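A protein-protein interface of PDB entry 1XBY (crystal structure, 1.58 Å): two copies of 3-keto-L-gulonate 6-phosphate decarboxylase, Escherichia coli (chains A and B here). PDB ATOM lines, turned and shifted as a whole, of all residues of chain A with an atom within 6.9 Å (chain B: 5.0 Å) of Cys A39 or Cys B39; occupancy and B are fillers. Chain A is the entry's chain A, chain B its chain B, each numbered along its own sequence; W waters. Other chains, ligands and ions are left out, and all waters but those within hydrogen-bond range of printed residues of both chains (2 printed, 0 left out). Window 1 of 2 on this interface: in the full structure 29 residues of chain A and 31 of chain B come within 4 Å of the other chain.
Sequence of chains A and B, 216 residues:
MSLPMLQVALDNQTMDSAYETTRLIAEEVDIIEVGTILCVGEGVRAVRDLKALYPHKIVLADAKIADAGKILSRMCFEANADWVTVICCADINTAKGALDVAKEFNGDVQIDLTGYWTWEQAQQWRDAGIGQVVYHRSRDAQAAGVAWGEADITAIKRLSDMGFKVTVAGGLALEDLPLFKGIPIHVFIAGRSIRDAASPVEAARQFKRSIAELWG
The backbone carbonyl oxygen (O) of Val B40 is in hydrogen-bond range of the backbone NH (N) of Val A44 (2.8 Å). O of Val A40 sits at hydrogen-bond distance from N of Val B44 (2.8 Å).
The backbone carbonyl oxygen (O) of Gly A35 sits at hydrogen-bond distance from the side-chain sulfur (SG) of Cys A39. The backbone carbonyl oxygen (O) of Gly B35 sits at hydrogen-bond distance from the side-chain sulfur (SG) of Cys B39.
Among the printed residues, pairs that only touch across the chains: Gly A43 with Val B40 (3.0 Å), Val A40 with Gly B43 (3.2 Å), Met A75 with Ile B37 (3.5 Å), Met A75 with Gly B41 (3.5 Å), Gly A43 with Gly B43 (3.7 Å), Gly A41 with Val B44 (3.7 Å), Glu A42 with Glu B42 (3.7 Å), Cys A39 with Cys B39 (3.9 Å), Val A44 with Gly B41 (3.9 Å), Glu A42 with Gly B43 (3.9 Å) and Gly A41 with Gly B43 (3.98 Å).
Cys A39 touches just one residue of chain B: Cys B39. Printed residues of chain B within 4 Å of Gly A43: Val B40 (3.0 Å) and Gly B43 (3.7 Å). Of the printed residues of chain B, Met A75 touches Ile B37 (3.5 Å) and Gly B41 (3.5 Å). Cys B39 touches just one residue of chain A: Cys A39. The nearest residue of chain B that does not touch Cys A39 is Gly B43 (4.3 Å). The nearest printed residue of chain A that does not touch Val B40 is Met A75 (4.2 Å).
Of the 14 printed residues of chain B, 7 touch a printed residue of chain A. Among the printed residues, no Asp or Glu carboxylate lies within 4 Å of a Lys or Arg side-chain nitrogen of the other chain.
Val A40 touches Gly B43, and with the chains exchanged Gly A43 touches Val B40. Val A40 touches Val B44, and with the chains exchanged Val A44 touches Val B40. Gly A41 touches Gly B43, but with the chains exchanged Gly A43 does not touch Gly B41 (4.2 Å). Glu A42 touches Gly B43, but with the chains exchanged Gly A43 does not touch Glu B42 (4.2 Å). Of the 13 pairs that touch across the chains among the printed residues, 9 have their exchanged pair printed and touching as well.
Water W2 lies within hydrogen-bond range of the backbone carbonyl oxygen of Gly B41 (2.7 Å), the backbone carbonyl oxygen of Glu A42 (2.8 Å) and the backbone NH of Val A44 (3.3 Å). Water W1 lies within hydrogen-bond range of the backbone carbonyl oxygen (O) of Gly A41 (2.7 Å), the backbone carbonyl oxygen (O) of Glu B42 (3.0 Å) and the backbone NH (N) of Val B44 (3.2 Å).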
ATOM      1  N   LEU A  10     -29.974  13.887 -32.879  1.00  0.00           N
ATOM      2  CA  LEU A  10     -29.019  13.893 -33.995  1.00  0.00           C
ATOM      3  C   LEU A  10     -27.996  12.800 -33.713  1.00  0.00           C
ATOM      4  O   LEU A  10     -26.908  13.059 -33.179  1.00  0.00           O
ATOM      5  CB  LEU A  10     -28.362  15.291 -34.145  1.00  0.00           C
ATOM      6  CG  LEU A  10     -29.310  16.453 -34.360  1.00  0.00           C
ATOM      7  CD1 LEU A  10     -28.630  17.748 -34.402  1.00  0.00           C
ATOM      8  CD2 LEU A  10     -30.126  16.245 -35.662  1.00  0.00           C
ATOM      9  N   ASN A  12     -25.983  11.123 -35.603  1.00  0.00           N
ATOM     10  CA  ASN A  12     -25.261  11.189 -36.877  1.00  0.00           C
ATOM     11  C   ASN A  12     -23.794  11.093 -36.598  1.00  0.00           C
ATOM     12  O   ASN A  12     -23.341  11.502 -35.545  1.00  0.00           O
ATOM     13  CB  ASN A  12     -25.503  12.541 -37.554  1.00  0.00           C
ATOM     14  CG  ASN A  12     -26.951  12.815 -37.844  1.00  0.00           C
ATOM     15  OD1 ASN A  12     -27.405  12.585 -38.967  1.00  0.00           O
ATOM     16  ND2 ASN A  12     -27.694  13.285 -36.859  1.00  0.00           N
ATOM     17  N   GLN A  13     -23.012  10.565 -37.536  1.00  0.00           N
ATOM     18  CA  GLN A  13     -21.584  10.398 -37.323  1.00  0.00           C
ATOM     19  C   GLN A  13     -20.731  11.632 -37.533  1.00  0.00           C
ATOM     20  O   GLN A  13     -19.631  11.722 -36.976  1.00  0.00           O
ATOM     21  CB  GLN A  13     -21.081   9.227 -38.157  1.00  0.00           C
ATOM     22  CG  GLN A  13     -21.708   7.962 -37.655  1.00  0.00           C
ATOM     23  CD  GLN A  13     -21.113   6.710 -38.239  1.00  0.00           C
ATOM     24  OE1 GLN A  13     -21.844   5.750 -38.470  1.00  0.00           O
ATOM     25  NE2 GLN A  13     -19.821   6.708 -38.472  1.00  0.00           N
ATOM     26  N   VAL A  34     -27.647  16.579 -29.405  1.00  0.00           N
ATOM     27  CA  VAL A  34     -26.399  16.042 -29.910  1.00  0.00           C
ATOM     28  C   VAL A  34     -26.363  14.586 -29.449  1.00  0.00           C
ATOM     29  O   VAL A  34     -26.124  14.263 -28.297  1.00  0.00           O
ATOM     30  CB  VAL A  34     -25.195  16.816 -29.385  1.00  0.00           C
ATOM     31  CG1 VAL A  34     -23.934  16.260 -29.976  1.00  0.00           C
ATOM     32  CG2 VAL A  34     -25.396  18.275 -29.687  1.00  0.00           C
ATOM     33  N   GLY A  35     -26.666  13.638 -30.320  1.00  0.00           N
ATOM     34  CA  GLY A  35     -26.745  12.270 -29.892  1.00  0.00           C
ATOM     35  C   GLY A  35     -25.425  11.711 -29.477  1.00  0.00           C
ATOM     36  O   GLY A  35     -24.360  12.231 -29.852  1.00  0.00           O
ATOM     37  N   THR A  36     -25.469  10.604 -28.765  1.00  0.00           N
ATOM     38  CA  THR A  36     -24.245   9.988 -28.299  1.00  0.00           C
ATOM     39  C   THR A  36     -23.350   9.652 -29.498  1.00  0.00           C
ATOM     40  O   THR A  36     -22.149   9.770 -29.461  1.00  0.00           O
ATOM     41  CB  THR A  36     -24.558   8.725 -27.514  1.00  0.00           C
ATOM     42  OG1 THR A  36     -25.625   8.951 -26.582  1.00  0.00           O
ATOM     43  CG2 THR A  36     -23.323   8.231 -26.753  1.00  0.00           C
ATOM     44  N   ILE A  37     -23.960   9.240 -30.599  1.00  0.00           N
ATOM     45  CA  ILE A  37     -23.251   8.887 -31.799  1.00  0.00           C
ATOM     46  C   ILE A  37     -22.500  10.114 -32.370  1.00  0.00           C
ATOM     47  O   ILE A  37     -21.366   9.976 -32.841  1.00  0.00           O
ATOM     48  CB  ILE A  37     -24.263   8.213 -32.764  1.00  0.00           C
ATOM     49  CG1 ILE A  37     -24.533   6.780 -32.241  1.00  0.00           C
ATOM     50  CG2 ILE A  37     -23.791   8.154 -34.206  1.00  0.00           C
ATOM     51  CD1 ILE A  37     -25.772   6.087 -32.853  1.00  0.00           C
ATOM     52  N   LEU A  38     -23.105  11.310 -32.270  1.00  0.00           N
ATOM     53  CA  LEU A  38     -22.478  12.508 -32.771  1.00  0.00           C
ATOM     54  C   LEU A  38     -21.392  12.979 -31.811  1.00  0.00           C
ATOM     55  O   LEU A  38     -20.371  13.409 -32.248  1.00  0.00           O
ATOM     56  CB  LEU A  38     -23.510  13.610 -32.998  1.00  0.00           C
ATOM     57  CG  LEU A  38     -23.046  14.865 -33.688  1.00  0.00           C
ATOM     58  CD1 LEU A  38     -22.321  14.594 -34.998  1.00  0.00           C
ATOM     59  CD2 LEU A  38     -24.236  15.787 -33.919  1.00  0.00           C
ATOM     60  N   CYS A  39     -21.637  12.800 -30.522  1.00  0.00           N
ATOM     61  CA  CYS A  39     -20.608  13.134 -29.494  1.00  0.00           C
ATOM     62  C   CYS A  39     -19.377  12.268 -29.753  1.00  0.00           C
ATOM     63  O   CYS A  39     -18.267  12.727 -29.696  1.00  0.00           O
ATOM     64  CB  CYS A  39     -21.130  12.804 -28.113  1.00  0.00           C
ATOM     65  SG  CYS A  39     -22.409  13.899 -27.421  1.00  0.00           S
ATOM     66  N   VAL A  40     -19.571  11.004 -30.100  1.00  0.00           N
ATOM     67  CA  VAL A  40     -18.424  10.115 -30.328  1.00  0.00           C
ATOM     68  C   VAL A  40     -17.787  10.363 -31.695  1.00  0.00           C
ATOM     69  O   VAL A  40     -16.573  10.243 -31.863  1.00  0.00           O
ATOM     70  CB  VAL A  40     -18.840   8.633 -30.186  1.00  0.00           C
ATOM     71  CG1 VAL A  40     -17.752   7.622 -30.680  1.00  0.00           C
ATOM     72  CG2 VAL A  40     -19.135   8.345 -28.736  1.00  0.00           C
ATOM     73  N   GLY A  41     -18.600  10.719 -32.682  1.00  0.00           N
ATOM     74  CA  GLY A  41     -18.120  10.955 -34.026  1.00  0.00           C
ATOM     75  C   GLY A  41     -17.283  12.242 -34.080  1.00  0.00           C
ATOM     76  O   GLY A  41     -16.193  12.252 -34.676  1.00  0.00           O
ATOM     77  N   GLU A  42     -17.788  13.334 -33.482  1.00  0.00           N
ATOM     78  CA  GLU A  42     -17.203  14.627 -33.667  1.00  0.00           C
ATOM     79  C   GLU A  42     -16.617  15.227 -32.362  1.00  0.00           C
ATOM     80  O   GLU A  42     -15.861  16.214 -32.423  1.00  0.00           O
ATOM     81  CB  GLU A  42     -18.224  15.593 -34.228  1.00  0.00           C
ATOM     82  CG  GLU A  42     -18.661  15.300 -35.658  1.00  0.00           C
ATOM     83  CD  GLU A  42     -17.677  15.774 -36.703  1.00  0.00           C
ATOM     84  OE1 GLU A  42     -16.473  16.070 -36.389  1.00  0.00           O
ATOM     85  OE2 GLU A  42     -18.130  15.961 -37.834  1.00  0.00           O
ATOM     86  N   GLY A  43     -17.014  14.712 -31.228  1.00  0.00           N
ATOM     87  CA  GLY A  43     -16.671  15.315 -29.935  1.00  0.00           C
ATOM     88  C   GLY A  43     -17.481  16.535 -29.651  1.00  0.00           C
ATOM     89  O   GLY A  43     -18.428  16.877 -30.346  1.00  0.00           O
ATOM     90  N   VAL A  44     -17.053  17.247 -28.632  1.00  0.00           N
ATOM     91  CA  VAL A  44     -17.831  18.305 -28.048  1.00  0.00           C
ATOM     92  C   VAL A  44     -17.983  19.512 -28.992  1.00  0.00           C
ATOM     93  O   VAL A  44     -18.836  20.390 -28.775  1.00  0.00           O
ATOM     94  CB  VAL A  44     -17.201  18.635 -26.675  1.00  0.00           C
ATOM     95  CG1 VAL A  44     -15.931  19.412 -26.792  1.00  0.00           C
ATOM     96  CG2 VAL A  44     -18.218  19.184 -25.809  1.00  0.00           C
ATOM     97  N   ALA A  46     -19.440  19.388 -31.568  1.00  0.00           N
ATOM     98  CA  ALA A  46     -20.797  19.245 -32.069  1.00  0.00           C
ATOM     99  C   ALA A  46     -21.771  20.093 -31.264  1.00  0.00           C
ATOM    100  O   ALA A  46     -22.671  20.698 -31.816  1.00  0.00           O
ATOM    101  CB  ALA A  46     -21.238  17.813 -31.992  1.00  0.00           C
ATOM    102  N   VAL A  47     -21.575  20.127 -29.958  1.00  0.00           N
ATOM    103  CA  VAL A  47     -22.404  20.888 -29.058  1.00  0.00           C
ATOM    104  C   VAL A  47     -22.188  22.383 -29.319  1.00  0.00           C
ATOM    105  O   VAL A  47     -23.141  23.136 -29.515  1.00  0.00           O
ATOM    106  CB  VAL A  47     -22.080  20.570 -27.572  1.00  0.00           C
ATOM    107  CG1 VAL A  47     -22.891  21.455 -26.659  1.00  0.00           C
ATOM    108  CG2 VAL A  47     -22.351  19.095 -27.238  1.00  0.00           C
ATOM    109  N   LEU A  60     -29.184  19.641 -25.936  1.00  0.00           N
ATOM    110  CA  LEU A  60     -28.885  18.547 -25.021  1.00  0.00           C
ATOM    111  C   LEU A  60     -27.697  17.758 -25.553  1.00  0.00           C
ATOM    112  O   LEU A  60     -27.675  17.372 -26.724  1.00  0.00           O
ATOM    113  CB  LEU A  60     -30.117  17.664 -24.804  1.00  0.00           C
ATOM    114  CG  LEU A  60     -30.084  16.339 -24.018  1.00  0.00           C
ATOM    115  CD1 LEU A  60     -29.528  15.154 -24.811  1.00  0.00           C
ATOM    116  CD2 LEU A  60     -29.382  16.376 -22.718  1.00  0.00           C
ATOM    117  N   ALA A  61     -26.702  17.525 -24.699  1.00  0.00           N
ATOM    118  CA  ALA A  61     -25.555  16.694 -25.089  1.00  0.00           C
ATOM    119  C   ALA A  61     -25.782  15.337 -24.479  1.00  0.00           C
ATOM    120  O   ALA A  61     -25.782  15.176 -23.257  1.00  0.00           O
ATOM    121  CB  ALA A  61     -24.252  17.316 -24.552  1.00  0.00           C
ATOM    122  N   ASP A  62     -26.090  14.353 -25.326  1.00  0.00           N
ATOM    123  CA  ASP A  62     -26.419  13.026 -24.845  1.00  0.00           C
ATOM    124  C   ASP A  62     -25.165  12.177 -24.609  1.00  0.00           C
ATOM    125  O   ASP A  62     -24.982  11.106 -25.225  1.00  0.00           O
ATOM    126  CB  ASP A  62     -27.404  12.329 -25.815  1.00  0.00           C
ATOM    127  CG  ASP A  62     -28.125  11.165 -25.185  1.00  0.00           C
ATOM    128  OD1 ASP A  62     -28.109  10.971 -23.950  1.00  0.00           O
ATOM    129  OD2 ASP A  62     -28.666  10.294 -25.911  1.00  0.00           O
ATOM    130  N   ALA A  63     -24.346  12.618 -23.667  1.00  0.00           N
ATOM    131  CA  ALA A  63     -23.051  12.022 -23.354  1.00  0.00           C
ATOM    132  C   ALA A  63     -23.153  10.731 -22.542  1.00  0.00           C
ATOM    133  O   ALA A  63     -22.238   9.946 -22.527  1.00  0.00           O
ATOM    134  CB  ALA A  63     -22.191  13.064 -22.624  1.00  0.00           C
ATOM    135  N   LYS A  64     -24.296  10.499 -21.922  1.00  0.00           N
ATOM    136  CA  LYS A  64     -24.544   9.346 -21.110  1.00  0.00           C
ATOM    137  C   LYS A  64     -23.351   9.057 -20.206  1.00  0.00           C
ATOM    138  O   LYS A  64     -22.785   7.986 -20.139  1.00  0.00           O
ATOM    139  CB  LYS A  64     -24.906   8.158 -21.993  1.00  0.00           C
ATOM    140  CG  LYS A  64     -26.287   8.375 -22.679  1.00  0.00           C
ATOM    141  CD  LYS A  64     -26.680   7.214 -23.644  1.00  0.00           C
ATOM    142  CE  LYS A  64     -28.003   7.570 -24.366  1.00  0.00           C
ATOM    143  NZ  LYS A  64     -28.181   6.667 -25.553  1.00  0.00           N
ATOM    144  N   MET A  75     -17.013  19.889 -19.761  1.00  0.00           N
ATOM    145  CA  MET A  75     -16.682  19.955 -21.192  1.00  0.00           C
ATOM    146  C   MET A  75     -17.925  20.253 -22.043  1.00  0.00           C
ATOM    147  O   MET A  75     -17.865  21.088 -22.925  1.00  0.00           O
ATOM    148  CB  MET A  75     -16.023  18.659 -21.661  1.00  0.00           C
ATOM    149  CG  MET A  75     -14.654  18.443 -21.067  1.00  0.00           C
ATOM    150  SD  MET A  75     -14.113  16.710 -21.372  1.00  0.00           S
ATOM    151  CE  MET A  75     -13.904  16.804 -23.131  1.00  0.00           C
ATOM    152  N   CYS A  76     -19.046  19.619 -21.723  1.00  0.00           N
ATOM    153  CA  CYS A  76     -20.291  19.891 -22.418  1.00  0.00           C
ATOM    154  C   CYS A  76     -20.826  21.293 -22.139  1.00  0.00           C
ATOM    155  O   CYS A  76     -21.256  21.985 -23.049  1.00  0.00           O
ATOM    156  CB  CYS A  76     -21.336  18.867 -22.059  1.00  0.00           C
ATOM    157  SG  CYS A  76     -20.923  17.182 -22.584  1.00  0.00           S
ATOM    158  N   VAL B  34      -7.585   5.370 -25.320  1.00  0.00           N
ATOM    159  CA  VAL B  34      -8.230   6.594 -25.649  1.00  0.00           C
ATOM    160  C   VAL B  34      -9.356   6.717 -24.652  1.00  0.00           C
ATOM    161  O   VAL B  34     -10.363   6.020 -24.634  1.00  0.00           O
ATOM    162  CB  VAL B  34      -8.805   6.548 -27.074  1.00  0.00           C
ATOM    163  CG1 VAL B  34      -9.467   7.881 -27.402  1.00  0.00           C
ATOM    164  CG2 VAL B  34      -7.743   6.248 -28.048  1.00  0.00           C
ATOM    165  N   GLY B  35      -9.128   7.565 -23.646  1.00  0.00           N
ATOM    166  CA  GLY B  35     -10.067   7.670 -22.583  1.00  0.00           C
ATOM    167  C   GLY B  35     -11.424   8.229 -23.023  1.00  0.00           C
ATOM    168  O   GLY B  35     -11.524   8.968 -24.005  1.00  0.00           O
ATOM    169  N   THR B  36     -12.432   7.993 -22.186  1.00  0.00           N
ATOM    170  CA  THR B  36     -13.725   8.548 -22.456  1.00  0.00           C
ATOM    171  C   THR B  36     -13.632  10.066 -22.638  1.00  0.00           C
ATOM    172  O   THR B  36     -14.312  10.644 -23.508  1.00  0.00           O
ATOM    173  CB  THR B  36     -14.692   8.251 -21.315  1.00  0.00           C
ATOM    174  OG1 THR B  36     -14.566   6.887 -20.900  1.00  0.00           O
ATOM    175  CG2 THR B  36     -16.146   8.437 -21.812  1.00  0.00           C
ATOM    176  N   ILE B  37     -12.811  10.727 -21.811  1.00  0.00           N
ATOM    177  CA  ILE B  37     -12.665  12.172 -21.894  1.00  0.00           C
ATOM    178  C   ILE B  37     -12.066  12.636 -23.226  1.00  0.00           C
ATOM    179  O   ILE B  37     -12.483  13.658 -23.769  1.00  0.00           O
ATOM    180  CB  ILE B  37     -11.854  12.712 -20.641  1.00  0.00           C
ATOM    181  CG1 ILE B  37     -12.760  12.658 -19.394  1.00  0.00           C
ATOM    182  CG2 ILE B  37     -11.286  14.069 -20.861  1.00  0.00           C
ATOM    183  CD1 ILE B  37     -11.965  12.576 -18.023  1.00  0.00           C
ATOM    184  N   LEU B  38     -11.143  11.854 -23.789  1.00  0.00           N
ATOM    185  CA  LEU B  38     -10.541  12.209 -25.060  1.00  0.00           C
ATOM    186  C   LEU B  38     -11.538  11.833 -26.188  1.00  0.00           C
ATOM    187  O   LEU B  38     -11.586  12.563 -27.165  1.00  0.00           O
ATOM    188  CB  LEU B  38      -9.215  11.500 -25.234  1.00  0.00           C
ATOM    189  CG  LEU B  38      -8.438  11.807 -26.494  1.00  0.00           C
ATOM    190  CD1 LEU B  38      -8.152  13.302 -26.631  1.00  0.00           C
ATOM    191  CD2 LEU B  38      -7.166  11.011 -26.470  1.00  0.00           C
ATOM    192  N   CYS B  39     -12.312  10.771 -26.028  1.00  0.00           N
ATOM    193  CA  CYS B  39     -13.353  10.443 -27.029  1.00  0.00           C
ATOM    194  C   CYS B  39     -14.362  11.585 -27.129  1.00  0.00           C
ATOM    195  O   CYS B  39     -14.764  12.008 -28.222  1.00  0.00           O
ATOM    196  CB  CYS B  39     -14.094   9.168 -26.668  1.00  0.00           C
ATOM    197  SG  CYS B  39     -13.170   7.609 -26.790  1.00  0.00           S
ATOM    198  N   VAL B  40     -14.751  12.120 -25.972  1.00  0.00           N
ATOM    199  CA  VAL B  40     -15.698  13.227 -25.956  1.00  0.00           C
ATOM    200  C   VAL B  40     -15.053  14.526 -26.418  1.00  0.00           C
ATOM    201  O   VAL B  40     -15.716  15.343 -27.082  1.00  0.00           O
ATOM    202  CB  VAL B  40     -16.406  13.359 -24.567  1.00  0.00           C
ATOM    203  CG1 VAL B  40     -17.238  14.648 -24.458  1.00  0.00           C
ATOM    204  CG2 VAL B  40     -17.275  12.160 -24.292  1.00  0.00           C
ATOM    205  N   GLY B  41     -13.783  14.766 -26.094  1.00  0.00           N
ATOM    206  CA  GLY B  41     -13.121  15.994 -26.458  1.00  0.00           C
ATOM    207  C   GLY B  41     -12.913  16.086 -27.968  1.00  0.00           C
ATOM    208  O   GLY B  41     -13.179  17.106 -28.572  1.00  0.00           O
ATOM    209  N   GLU B  42     -12.462  14.995 -28.559  1.00  0.00           N
ATOM    210  CA  GLU B  42     -12.003  15.037 -29.938  1.00  0.00           C
ATOM    211  C   GLU B  42     -12.787  14.170 -30.878  1.00  0.00           C
ATOM    212  O   GLU B  42     -12.641  14.335 -32.098  1.00  0.00           O
ATOM    213  CB  GLU B  42     -10.563  14.572 -30.005  1.00  0.00           C
ATOM    214  CG  GLU B  42      -9.564  15.526 -29.422  1.00  0.00           C
ATOM    215  CD  GLU B  42      -9.201  16.709 -30.262  1.00  0.00           C
ATOM    216  OE1 GLU B  42      -9.893  17.005 -31.263  1.00  0.00           O
ATOM    217  OE2 GLU B  42      -8.159  17.341 -29.944  1.00  0.00           O
ATOM    218  N   GLY B  43     -13.595  13.270 -30.364  1.00  0.00           N
ATOM    219  CA  GLY B  43     -14.263  12.280 -31.197  1.00  0.00           C
ATOM    220  C   GLY B  43     -13.335  11.167 -31.646  1.00  0.00           C
ATOM    221  O   GLY B  43     -12.176  11.062 -31.268  1.00  0.00           O
ATOM    222  N   VAL B  44     -13.873  10.306 -32.485  1.00  0.00           N
ATOM    223  CA  VAL B  44     -13.212   9.053 -32.811  1.00  0.00           C
ATOM    224  C   VAL B  44     -11.913   9.230 -33.649  1.00  0.00           C
ATOM    225  O   VAL B  44     -11.102   8.303 -33.789  1.00  0.00           O
ATOM    226  CB  VAL B  44     -14.233   8.119 -33.443  1.00  0.00           C
ATOM    227  CG1 VAL B  44     -14.473   8.487 -34.865  1.00  0.00           C
ATOM    228  CG2 VAL B  44     -13.846   6.706 -33.248  1.00  0.00           C
ATOM    229  N   ALA B  61     -10.555   1.884 -27.133  1.00  0.00           N
ATOM    230  CA  ALA B  61     -11.432   3.057 -27.104  1.00  0.00           C
ATOM    231  C   ALA B  61     -12.363   2.918 -25.946  1.00  0.00           C
ATOM    232  O   ALA B  61     -13.211   2.058 -25.899  1.00  0.00           O
ATOM    233  CB  ALA B  61     -12.223   3.158 -28.369  1.00  0.00           C
ATOM    234  N   ASP B  62     -12.233   3.755 -24.923  1.00  0.00           N
ATOM    235  CA  ASP B  62     -13.019   3.601 -23.733  1.00  0.00           C
ATOM    236  C   ASP B  62     -14.342   4.354 -23.826  1.00  0.00           C
ATOM    237  O   ASP B  62     -14.648   5.331 -23.156  1.00  0.00           O
ATOM    238  CB  ASP B  62     -12.197   4.085 -22.521  1.00  0.00           C
ATOM    239  CG  ASP B  62     -12.789   3.650 -21.203  1.00  0.00           C
ATOM    240  OD1 ASP B  62     -13.647   2.774 -21.129  1.00  0.00           O
ATOM    241  OD2 ASP B  62     -12.462   4.221 -20.125  1.00  0.00           O
ATOM    242  N   ALA B  63     -15.182   3.894 -24.756  1.00  0.00           N
ATOM    243  CA  ALA B  63     -16.366   4.581 -25.093  1.00  0.00           C
ATOM    244  C   ALA B  63     -17.516   4.360 -24.108  1.00  0.00           C
ATOM    245  O   ALA B  63     -18.459   5.145 -24.071  1.00  0.00           O
ATOM    246  CB  ALA B  63     -16.798   4.146 -26.518  1.00  0.00           C
HETATM  247  O   HOH W   1     -13.523  12.794 -34.523  1.00  0.00           O
HETATM  248  O   HOH W   2     -14.622  18.048 -30.676  1.00  0.00           O
